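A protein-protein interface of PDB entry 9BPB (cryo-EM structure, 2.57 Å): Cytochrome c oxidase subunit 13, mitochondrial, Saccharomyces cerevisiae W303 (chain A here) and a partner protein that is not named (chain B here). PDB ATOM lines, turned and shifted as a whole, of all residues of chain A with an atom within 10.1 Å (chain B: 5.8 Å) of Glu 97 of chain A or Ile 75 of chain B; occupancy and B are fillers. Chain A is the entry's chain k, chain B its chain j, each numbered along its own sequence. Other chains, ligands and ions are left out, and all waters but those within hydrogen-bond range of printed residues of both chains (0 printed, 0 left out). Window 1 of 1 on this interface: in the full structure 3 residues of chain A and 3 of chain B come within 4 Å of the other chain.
The backbone carbonyl oxygen (O) of Ile 75 of chain B lies close to the side-chain carboxylate (OE1) of Glu 97 of chain A.
The backbone carbonyl oxygen of Gln 70 of chain B sits at hydrogen-bond distance from the backbone NH of Ile 75 of chain B. The backbone carbonyl oxygen of Gln 70 of chain B lies within hydrogen-bond range of the backbone NH of Phe 76 of chain B, 3.2 Å away. The side-chain carboxylate (OD2) of Asp 95 of chain A sits at hydrogen-bond distance from the side-chain amide nitrogen (ND2) of Asn 100 of chain A, 3.3 Å away.
Asp 95 of chain A touches Ile 75 of chain B. O of Ile 75 of chain B touches CD2 of Tyr 96 of chain A, 3.1 Å away. CE2 of Tyr 96 of chain A touches O of Phe 76 of chain B, at 3.8 Å. CD of Glu 97 of chain A touches OE1 of Gln 70 of chain B, at 3.5 Å.
Of the printed residues of chain B, Asp 95 of chain A touches Ile 75 (3.3 Å). Of the printed residues of chain B, Tyr 96 of chain A touches Ile 75 (3.1 Å) and Phe 76 (3.8 Å). Glu 97 of chain A touches just these residues of chain B: Gln 70 (3.5 Å) and Ile 75 (3.3 Å). Of chain A, only Glu 97 (3.5 Å) comes within 4 Å of Gln 70 of chain B. No residue of chain A comes within 4 Å of Lys 73 of chain B. Of chain A, only Asp 95 (3.3 Å), Tyr 96 (3.1 Å) and Glu 97 (3.3 Å) come within 4 Å of Ile 75 of chain B. Printed residues of chain A within 4 Å of Phe 76 of chain B: Tyr 96. The nearest residue of chain B that does not touch Glu 97 of chain A is Ala 77 of chain B (4.6 Å). The nearest residue of chain A that does not touch Ile 75 of chain B is Arg 94 of chain A (4.5 Å). The nearest printed residue of chain B that does not touch Asp 95 of chain A is Gly 74 of chain B (7.0 Å).
Hydrophobic or aromatic side chains of chain B that line the printed part of chain A: Ile 75. Along chain B the printed residues that touch a printed residue of chain A span positions 70 to 76. Of the 14 printed residues of chain A, 3 touch a printed residue of chain B. Hydrophobic or aromatic side chains of chain A within 4 Å of the printed part of chain B: Tyr 96. Among the printed residues, no Asp or Glu carboxylate lies within 4 Å of a Lys or Arg side-chain nitrogen of the other chain.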
ATOM      1  N   TRP A  92      -6.271  -3.483  20.881  1.00  0.00           N
ATOM      2  CA  TRP A  92      -6.005  -2.555  21.976  1.00  0.00           C
ATOM      3  C   TRP A  92      -7.300  -2.136  22.661  1.00  0.00           C
ATOM      4  O   TRP A  92      -8.341  -2.017  21.999  1.00  0.00           O
ATOM      5  CB  TRP A  92      -5.269  -1.327  21.436  1.00  0.00           C
ATOM      6  CG  TRP A  92      -4.272  -0.713  22.366  1.00  0.00           C
ATOM      7  CD1 TRP A  92      -4.293   0.557  22.860  1.00  0.00           C
ATOM      8  CD2 TRP A  92      -3.093  -1.329  22.891  1.00  0.00           C
ATOM      9  NE1 TRP A  92      -3.207   0.767  23.672  1.00  0.00           N
ATOM     10  CE2 TRP A  92      -2.452  -0.376  23.707  1.00  0.00           C
ATOM     11  CE3 TRP A  92      -2.517  -2.596  22.755  1.00  0.00           C
ATOM     12  CZ2 TRP A  92      -1.268  -0.650  24.385  1.00  0.00           C
ATOM     13  CZ3 TRP A  92      -1.342  -2.865  23.429  1.00  0.00           C
ATOM     14  CH2 TRP A  92      -0.729  -1.897  24.233  1.00  0.00           C
ATOM     15  N   PRO A  93      -7.285  -1.915  23.976  1.00  0.00           N
ATOM     16  CA  PRO A  93      -8.519  -1.541  24.675  1.00  0.00           C
ATOM     17  C   PRO A  93      -9.122  -0.268  24.100  1.00  0.00           C
ATOM     18  O   PRO A  93      -8.410   0.670  23.737  1.00  0.00           O
ATOM     19  CB  PRO A  93      -8.059  -1.338  26.123  1.00  0.00           C
ATOM     20  CG  PRO A  93      -6.810  -2.145  26.239  1.00  0.00           C
ATOM     21  CD  PRO A  93      -6.149  -2.074  24.899  1.00  0.00           C
ATOM     22  N   ARG A  94     -10.449  -0.245  24.018  1.00  0.00           N
ATOM     23  CA  ARG A  94     -11.138   0.889  23.426  1.00  0.00           C
ATOM     24  C   ARG A  94     -11.026   2.113  24.327  1.00  0.00           C
ATOM     25  O   ARG A  94     -10.789   2.009  25.533  1.00  0.00           O
ATOM     26  CB  ARG A  94     -12.605   0.553  23.168  1.00  0.00           C
ATOM     27  CG  ARG A  94     -12.818  -0.388  21.991  1.00  0.00           C
ATOM     28  CD  ARG A  94     -14.225  -0.273  21.428  1.00  0.00           C
ATOM     29  NE  ARG A  94     -14.490   1.052  20.879  1.00  0.00           N
ATOM     30  CZ  ARG A  94     -15.408   1.311  19.957  1.00  0.00           C
ATOM     31  NH1 ARG A  94     -16.165   0.354  19.447  1.00  0.00           N
ATOM     32  NH2 ARG A  94     -15.569   2.561  19.534  1.00  0.00           N
ATOM     33  N   ASP A  95     -11.201   3.284  23.725  1.00  0.00           N
ATOM     34  CA  ASP A  95     -10.963   4.554  24.394  1.00  0.00           C
ATOM     35  C   ASP A  95     -12.283   5.184  24.818  1.00  0.00           C
ATOM     36  O   ASP A  95     -13.241   5.216  24.040  1.00  0.00           O
ATOM     37  CB  ASP A  95     -10.199   5.508  23.475  1.00  0.00           C
ATOM     38  CG  ASP A  95      -8.838   4.973  23.087  1.00  0.00           C
ATOM     39  OD1 ASP A  95      -8.239   4.229  23.891  1.00  0.00           O
ATOM     40  OD2 ASP A  95      -8.363   5.302  21.981  1.00  0.00           O
ATOM     41  N   TYR A  96     -12.321   5.688  26.048  1.00  0.00           N
ATOM     42  CA  TYR A  96     -13.486   6.413  26.527  1.00  0.00           C
ATOM     43  C   TYR A  96     -13.594   7.759  25.812  1.00  0.00           C
ATOM     44  O   TYR A  96     -12.699   8.181  25.076  1.00  0.00           O
ATOM     45  CB  TYR A  96     -13.407   6.609  28.039  1.00  0.00           C
ATOM     46  CG  TYR A  96     -13.639   5.344  28.833  1.00  0.00           C
ATOM     47  CD1 TYR A  96     -12.623   4.417  29.011  1.00  0.00           C
ATOM     48  CD2 TYR A  96     -14.876   5.076  29.398  1.00  0.00           C
ATOM     49  CE1 TYR A  96     -12.831   3.260  29.731  1.00  0.00           C
ATOM     50  CE2 TYR A  96     -15.095   3.920  30.119  1.00  0.00           C
ATOM     51  CZ  TYR A  96     -14.071   3.017  30.283  1.00  0.00           C
ATOM     52  OH  TYR A  96     -14.288   1.866  31.002  1.00  0.00           O
ATOM     53  N   GLU A  97     -14.721   8.438  26.038  1.00  0.00           N
ATOM     54  CA  GLU A  97     -14.993   9.677  25.319  1.00  0.00           C
ATOM     55  C   GLU A  97     -13.979  10.769  25.634  1.00  0.00           C
ATOM     56  O   GLU A  97     -13.855  11.724  24.859  1.00  0.00           O
ATOM     57  CB  GLU A  97     -16.409  10.172  25.628  1.00  0.00           C
ATOM     58  CG  GLU A  97     -16.673  10.491  27.094  1.00  0.00           C
ATOM     59  CD  GLU A  97     -17.079   9.274  27.908  1.00  0.00           C
ATOM     60  OE1 GLU A  97     -16.881   8.137  27.430  1.00  0.00           O
ATOM     61  OE2 GLU A  97     -17.601   9.457  29.028  1.00  0.00           O
ATOM     62  N   PHE A  98     -13.253  10.655  26.743  1.00  0.00           N
ATOM     63  CA  PHE A  98     -12.272  11.654  27.137  1.00  0.00           C
ATOM     64  C   PHE A  98     -10.838  11.215  26.889  1.00  0.00           C
ATOM     65  O   PHE A  98      -9.912  11.891  27.346  1.00  0.00           O
ATOM     66  CB  PHE A  98     -12.439  12.008  28.621  1.00  0.00           C
ATOM     67  CG  PHE A  98     -12.512  10.813  29.535  1.00  0.00           C
ATOM     68  CD1 PHE A  98     -11.363  10.292  30.102  1.00  0.00           C
ATOM     69  CD2 PHE A  98     -13.726  10.229  29.845  1.00  0.00           C
ATOM     70  CE1 PHE A  98     -11.422   9.201  30.949  1.00  0.00           C
ATOM     71  CE2 PHE A  98     -13.792   9.139  30.691  1.00  0.00           C
ATOM     72  CZ  PHE A  98     -12.637   8.625  31.241  1.00  0.00           C
ATOM     73  N   MET A  99     -10.625  10.113  26.169  1.00  0.00           N
ATOM     74  CA  MET A  99      -9.317   9.467  26.185  1.00  0.00           C
ATOM     75  C   MET A  99      -8.319  10.193  25.292  1.00  0.00           C
ATOM     76  O   MET A  99      -7.289  10.679  25.766  1.00  0.00           O
ATOM     77  CB  MET A  99      -9.453   8.003  25.776  1.00  0.00           C
ATOM     78  CG  MET A  99      -8.271   7.143  26.178  1.00  0.00           C
ATOM     79  SD  MET A  99      -8.104   6.991  27.965  1.00  0.00           S
ATOM     80  CE  MET A  99      -9.458   5.887  28.339  1.00  0.00           C
ATOM     81  N   ASN A 100      -8.592  10.273  23.995  1.00  0.00           N
ATOM     82  CA  ASN A 100      -7.700  10.957  23.064  1.00  0.00           C
ATOM     83  C   ASN A 100      -8.414  12.184  22.513  1.00  0.00           C
ATOM     84  O   ASN A 100      -9.452  12.058  21.854  1.00  0.00           O
ATOM     85  CB  ASN A 100      -7.260  10.026  21.936  1.00  0.00           C
ATOM     86  CG  ASN A 100      -6.110   9.121  22.342  1.00  0.00           C
ATOM     87  OD1 ASN A 100      -4.950   9.529  22.328  1.00  0.00           O
ATOM     88  ND2 ASN A 100      -6.429   7.885  22.705  1.00  0.00           N
ATOM     89  N   ILE A 101      -7.853  13.362  22.774  1.00  0.00           N
ATOM     90  CA  ILE A 101      -8.471  14.634  22.417  1.00  0.00           C
ATOM     91  C   ILE A 101      -7.703  15.217  21.241  1.00  0.00           C
ATOM     92  O   ILE A 101      -6.500  15.489  21.347  1.00  0.00           O
ATOM     93  CB  ILE A 101      -8.484  15.607  23.606  1.00  0.00           C
ATOM     94  CG1 ILE A 101      -9.330  15.043  24.748  1.00  0.00           C
ATOM     95  CG2 ILE A 101      -9.007  16.964  23.176  1.00  0.00           C
ATOM     96  CD1 ILE A 101     -10.765  14.774  24.370  1.00  0.00           C
ATOM     97  N   ARG A 102      -8.399  15.424  20.125  1.00  0.00           N
ATOM     98  CA  ARG A 102      -7.799  15.894  18.879  1.00  0.00           C
ATOM     99  C   ARG A 102      -8.545  17.114  18.353  1.00  0.00           C
ATOM    100  O   ARG A 102      -8.931  17.184  17.184  1.00  0.00           O
ATOM    101  CB  ARG A 102      -7.781  14.782  17.835  1.00  0.00           C
ATOM    102  CG  ARG A 102      -7.013  13.546  18.266  1.00  0.00           C
ATOM    103  CD  ARG A 102      -5.517  13.806  18.307  1.00  0.00           C
ATOM    104  NE  ARG A 102      -4.776  12.624  18.733  1.00  0.00           N
ATOM    105  CZ  ARG A 102      -3.955  12.588  19.774  1.00  0.00           C
ATOM    106  NH1 ARG A 102      -3.744  13.657  20.524  1.00  0.00           N
ATOM    107  NH2 ARG A 102      -3.334  11.451  20.071  1.00  0.00           N
ATOM    108  N   SER A 103      -8.768  18.100  19.227  1.00  0.00           N
ATOM    109  CA  SER A 103      -9.489  19.301  18.819  1.00  0.00           C
ATOM    110  C   SER A 103      -8.734  20.060  17.736  1.00  0.00           C
ATOM    111  O   SER A 103      -9.337  20.552  16.776  1.00  0.00           O
ATOM    112  CB  SER A 103      -9.739  20.198  20.031  1.00  0.00           C
ATOM    113  OG  SER A 103      -8.520  20.668  20.579  1.00  0.00           O
ATOM    114  N   HIS A 124      -3.402   4.877  20.004  1.00  0.00           N
ATOM    115  CA  HIS A 124      -4.453   5.719  19.424  1.00  0.00           C
ATOM    116  C   HIS A 124      -5.006   5.112  18.132  1.00  0.00           C
ATOM    117  O   HIS A 124      -4.852   5.659  17.037  1.00  0.00           O
ATOM    118  CB  HIS A 124      -3.967   7.153  19.187  1.00  0.00           C
ATOM    119  CG  HIS A 124      -5.038   8.073  18.686  1.00  0.00           C
ATOM    120  ND1 HIS A 124      -6.378   7.857  18.931  1.00  0.00           N
ATOM    121  CD2 HIS A 124      -4.970   9.207  17.947  1.00  0.00           C
ATOM    122  CE1 HIS A 124      -7.087   8.819  18.369  1.00  0.00           C
ATOM    123  NE2 HIS A 124      -6.257   9.650  17.765  1.00  0.00           N
ATOM    124  N   HIS A 127     -11.605   3.588  16.038  1.00  0.00           N
ATOM    125  CA  HIS A 127     -12.661   2.602  15.810  1.00  0.00           C
ATOM    126  C   HIS A 127     -13.820   3.298  15.105  1.00  0.00           C
ATOM    127  O   HIS A 127     -14.718   3.849  15.741  1.00  0.00           O
ATOM    128  CB  HIS A 127     -13.109   1.966  17.118  1.00  0.00           C
ATOM    129  CG  HIS A 127     -12.122   0.999  17.692  1.00  0.00           C
ATOM    130  ND1 HIS A 127     -12.193  -0.358  17.463  1.00  0.00           N
ATOM    131  CD2 HIS A 127     -11.047   1.190  18.493  1.00  0.00           C
ATOM    132  CE1 HIS A 127     -11.202  -0.962  18.093  1.00  0.00           C
ATOM    133  NE2 HIS A 127     -10.493  -0.044  18.726  1.00  0.00           N
ATOM    134  N   ASP B  69     -25.118   5.777  23.324  1.00  0.00           N
ATOM    135  CA  ASP B  69     -24.065   5.299  22.432  1.00  0.00           C
ATOM    136  C   ASP B  69     -22.849   4.830  23.219  1.00  0.00           C
ATOM    137  O   ASP B  69     -22.235   3.813  22.877  1.00  0.00           O
ATOM    138  CB  ASP B  69     -23.669   6.394  21.444  1.00  0.00           C
ATOM    139  CG  ASP B  69     -24.809   6.798  20.535  1.00  0.00           C
ATOM    140  OD1 ASP B  69     -25.421   5.904  19.916  1.00  0.00           O
ATOM    141  OD2 ASP B  69     -25.089   8.010  20.436  1.00  0.00           O
ATOM    142  N   GLN B  70     -22.445   5.580  24.237  1.00  0.00           N
ATOM    143  CA  GLN B  70     -21.259   5.205  25.045  1.00  0.00           C
ATOM    144  C   GLN B  70     -21.536   3.897  25.790  1.00  0.00           C
ATOM    145  O   GLN B  70     -20.612   3.088  25.903  1.00  0.00           O
ATOM    146  CB  GLN B  70     -20.922   6.325  26.024  1.00  0.00           C
ATOM    147  CG  GLN B  70     -20.452   7.606  25.363  1.00  0.00           C
ATOM    148  CD  GLN B  70     -20.404   8.711  26.386  1.00  0.00           C
ATOM    149  OE1 GLN B  70     -20.032   9.841  26.091  1.00  0.00           O
ATOM    150  NE2 GLN B  70     -20.787   8.382  27.608  1.00  0.00           N
ATOM    151  N   ARG B  71     -22.732   3.722  26.341  1.00  0.00           N
ATOM    152  CA  ARG B  71     -23.031   2.410  26.974  1.00  0.00           C
ATOM    153  C   ARG B  71     -22.897   1.319  25.913  1.00  0.00           C
ATOM    154  O   ARG B  71     -22.141   0.361  26.154  1.00  0.00           O
ATOM    155  CB  ARG B  71     -24.431   2.394  27.593  1.00  0.00           C
ATOM    156  CG  ARG B  71     -24.685   1.239  28.549  1.00  0.00           C
ATOM    157  CD  ARG B  71     -26.116   1.309  29.045  1.00  0.00           C
ATOM    158  NE  ARG B  71     -27.025   1.359  27.911  1.00  0.00           N
ATOM    159  CZ  ARG B  71     -27.805   2.391  27.614  1.00  0.00           C
ATOM    160  NH1 ARG B  71     -28.095   2.655  26.353  1.00  0.00           N
ATOM    161  NH2 ARG B  71     -28.268   3.172  28.573  1.00  0.00           N
ATOM    162  N   GLU B  72     -23.593   1.465  24.783  1.00  0.00           N
ATOM    163  CA  GLU B  72     -23.593   0.391  23.760  1.00  0.00           C
ATOM    164  C   GLU B  72     -22.157   0.042  23.388  1.00  0.00           C
ATOM    165  O   GLU B  72     -21.811  -1.149  23.434  1.00  0.00           O
ATOM    166  CB  GLU B  72     -24.310   0.863  22.501  1.00  0.00           C
ATOM    167  CG  GLU B  72     -24.632  -0.249  21.519  1.00  0.00           C
ATOM    168  CD  GLU B  72     -23.455  -0.763  20.710  1.00  0.00           C
ATOM    169  OE1 GLU B  72     -22.829   0.050  20.004  1.00  0.00           O
ATOM    170  OE2 GLU B  72     -23.164  -1.972  20.790  1.00  0.00           O
ATOM    171  N   LYS B  73     -21.353   1.042  23.041  1.00  0.00           N
ATOM    172  CA  LYS B  73     -19.986   0.796  22.599  1.00  0.00           C
ATOM    173  C   LYS B  73     -19.103   0.215  23.694  1.00  0.00           C
ATOM    174  O   LYS B  73     -17.989  -0.225  23.396  1.00  0.00           O
ATOM    175  CB  LYS B  73     -19.364   2.092  22.078  1.00  0.00           C
ATOM    176  CG  LYS B  73     -20.048   2.657  20.847  1.00  0.00           C
ATOM    177  CD  LYS B  73     -19.433   3.981  20.434  1.00  0.00           C
ATOM    178  CE  LYS B  73     -20.182   4.593  19.262  1.00  0.00           C
ATOM    179  NZ  LYS B  73     -19.607   5.901  18.853  1.00  0.00           N
ATOM    180  N   GLY B  74     -19.564   0.203  24.940  1.00  0.00           N
ATOM    181  CA  GLY B  74     -18.774  -0.306  26.038  1.00  0.00           C
ATOM    182  C   GLY B  74     -17.892   0.713  26.724  1.00  0.00           C
ATOM    183  O   GLY B  74     -17.014   0.321  27.501  1.00  0.00           O
ATOM    184  N   ILE B  75     -18.094   2.001  26.467  1.00  0.00           N
ATOM    185  CA  ILE B  75     -17.269   3.050  27.047  1.00  0.00           C
ATOM    186  C   ILE B  75     -18.060   3.895  28.045  1.00  0.00           C
ATOM    187  O   ILE B  75     -17.751   5.068  28.243  1.00  0.00           O
ATOM    188  CB  ILE B  75     -16.632   3.927  25.958  1.00  0.00           C
ATOM    189  CG1 ILE B  75     -17.669   4.303  24.900  1.00  0.00           C
ATOM    190  CG2 ILE B  75     -15.461   3.206  25.316  1.00  0.00           C
ATOM    191  CD1 ILE B  75     -17.192   5.361  23.933  1.00  0.00           C
ATOM    192  N   PHE B  76     -19.079   3.319  28.673  1.00  0.00           N
ATOM    193  CA  PHE B  76     -19.829   4.041  29.691  1.00  0.00           C
ATOM    194  C   PHE B  76     -19.004   4.147  30.969  1.00  0.00           C
ATOM    195  O   PHE B  76     -18.504   3.141  31.483  1.00  0.00           O
ATOM    196  CB  PHE B  76     -21.157   3.338  29.964  1.00  0.00           C
ATOM    197  CG  PHE B  76     -22.152   4.180  30.712  1.00  0.00           C
ATOM    198  CD1 PHE B  76     -22.348   5.507  30.379  1.00  0.00           C
ATOM    199  CD2 PHE B  76     -22.904   3.638  31.738  1.00  0.00           C
ATOM    200  CE1 PHE B  76     -23.265   6.280  31.063  1.00  0.00           C
ATOM    201  CE2 PHE B  76     -23.823   4.406  32.424  1.00  0.00           C
ATOM    202  CZ  PHE B  76     -24.004   5.727  32.084  1.00  0.00           C
ATOM    203  N   ALA B  77     -18.857   5.371  31.480  1.00  0.00           N
ATOM    204  CA  ALA B  77     -18.061   5.580  32.684  1.00  0.00           C
ATOM    205  C   ALA B  77     -18.706   4.930  33.902  1.00  0.00           C
ATOM    206  O   ALA B  77     -18.012   4.338  34.738  1.00  0.00           O
ATOM    207  CB  ALA B  77     -17.853   7.073  32.924  1.00  0.00           C
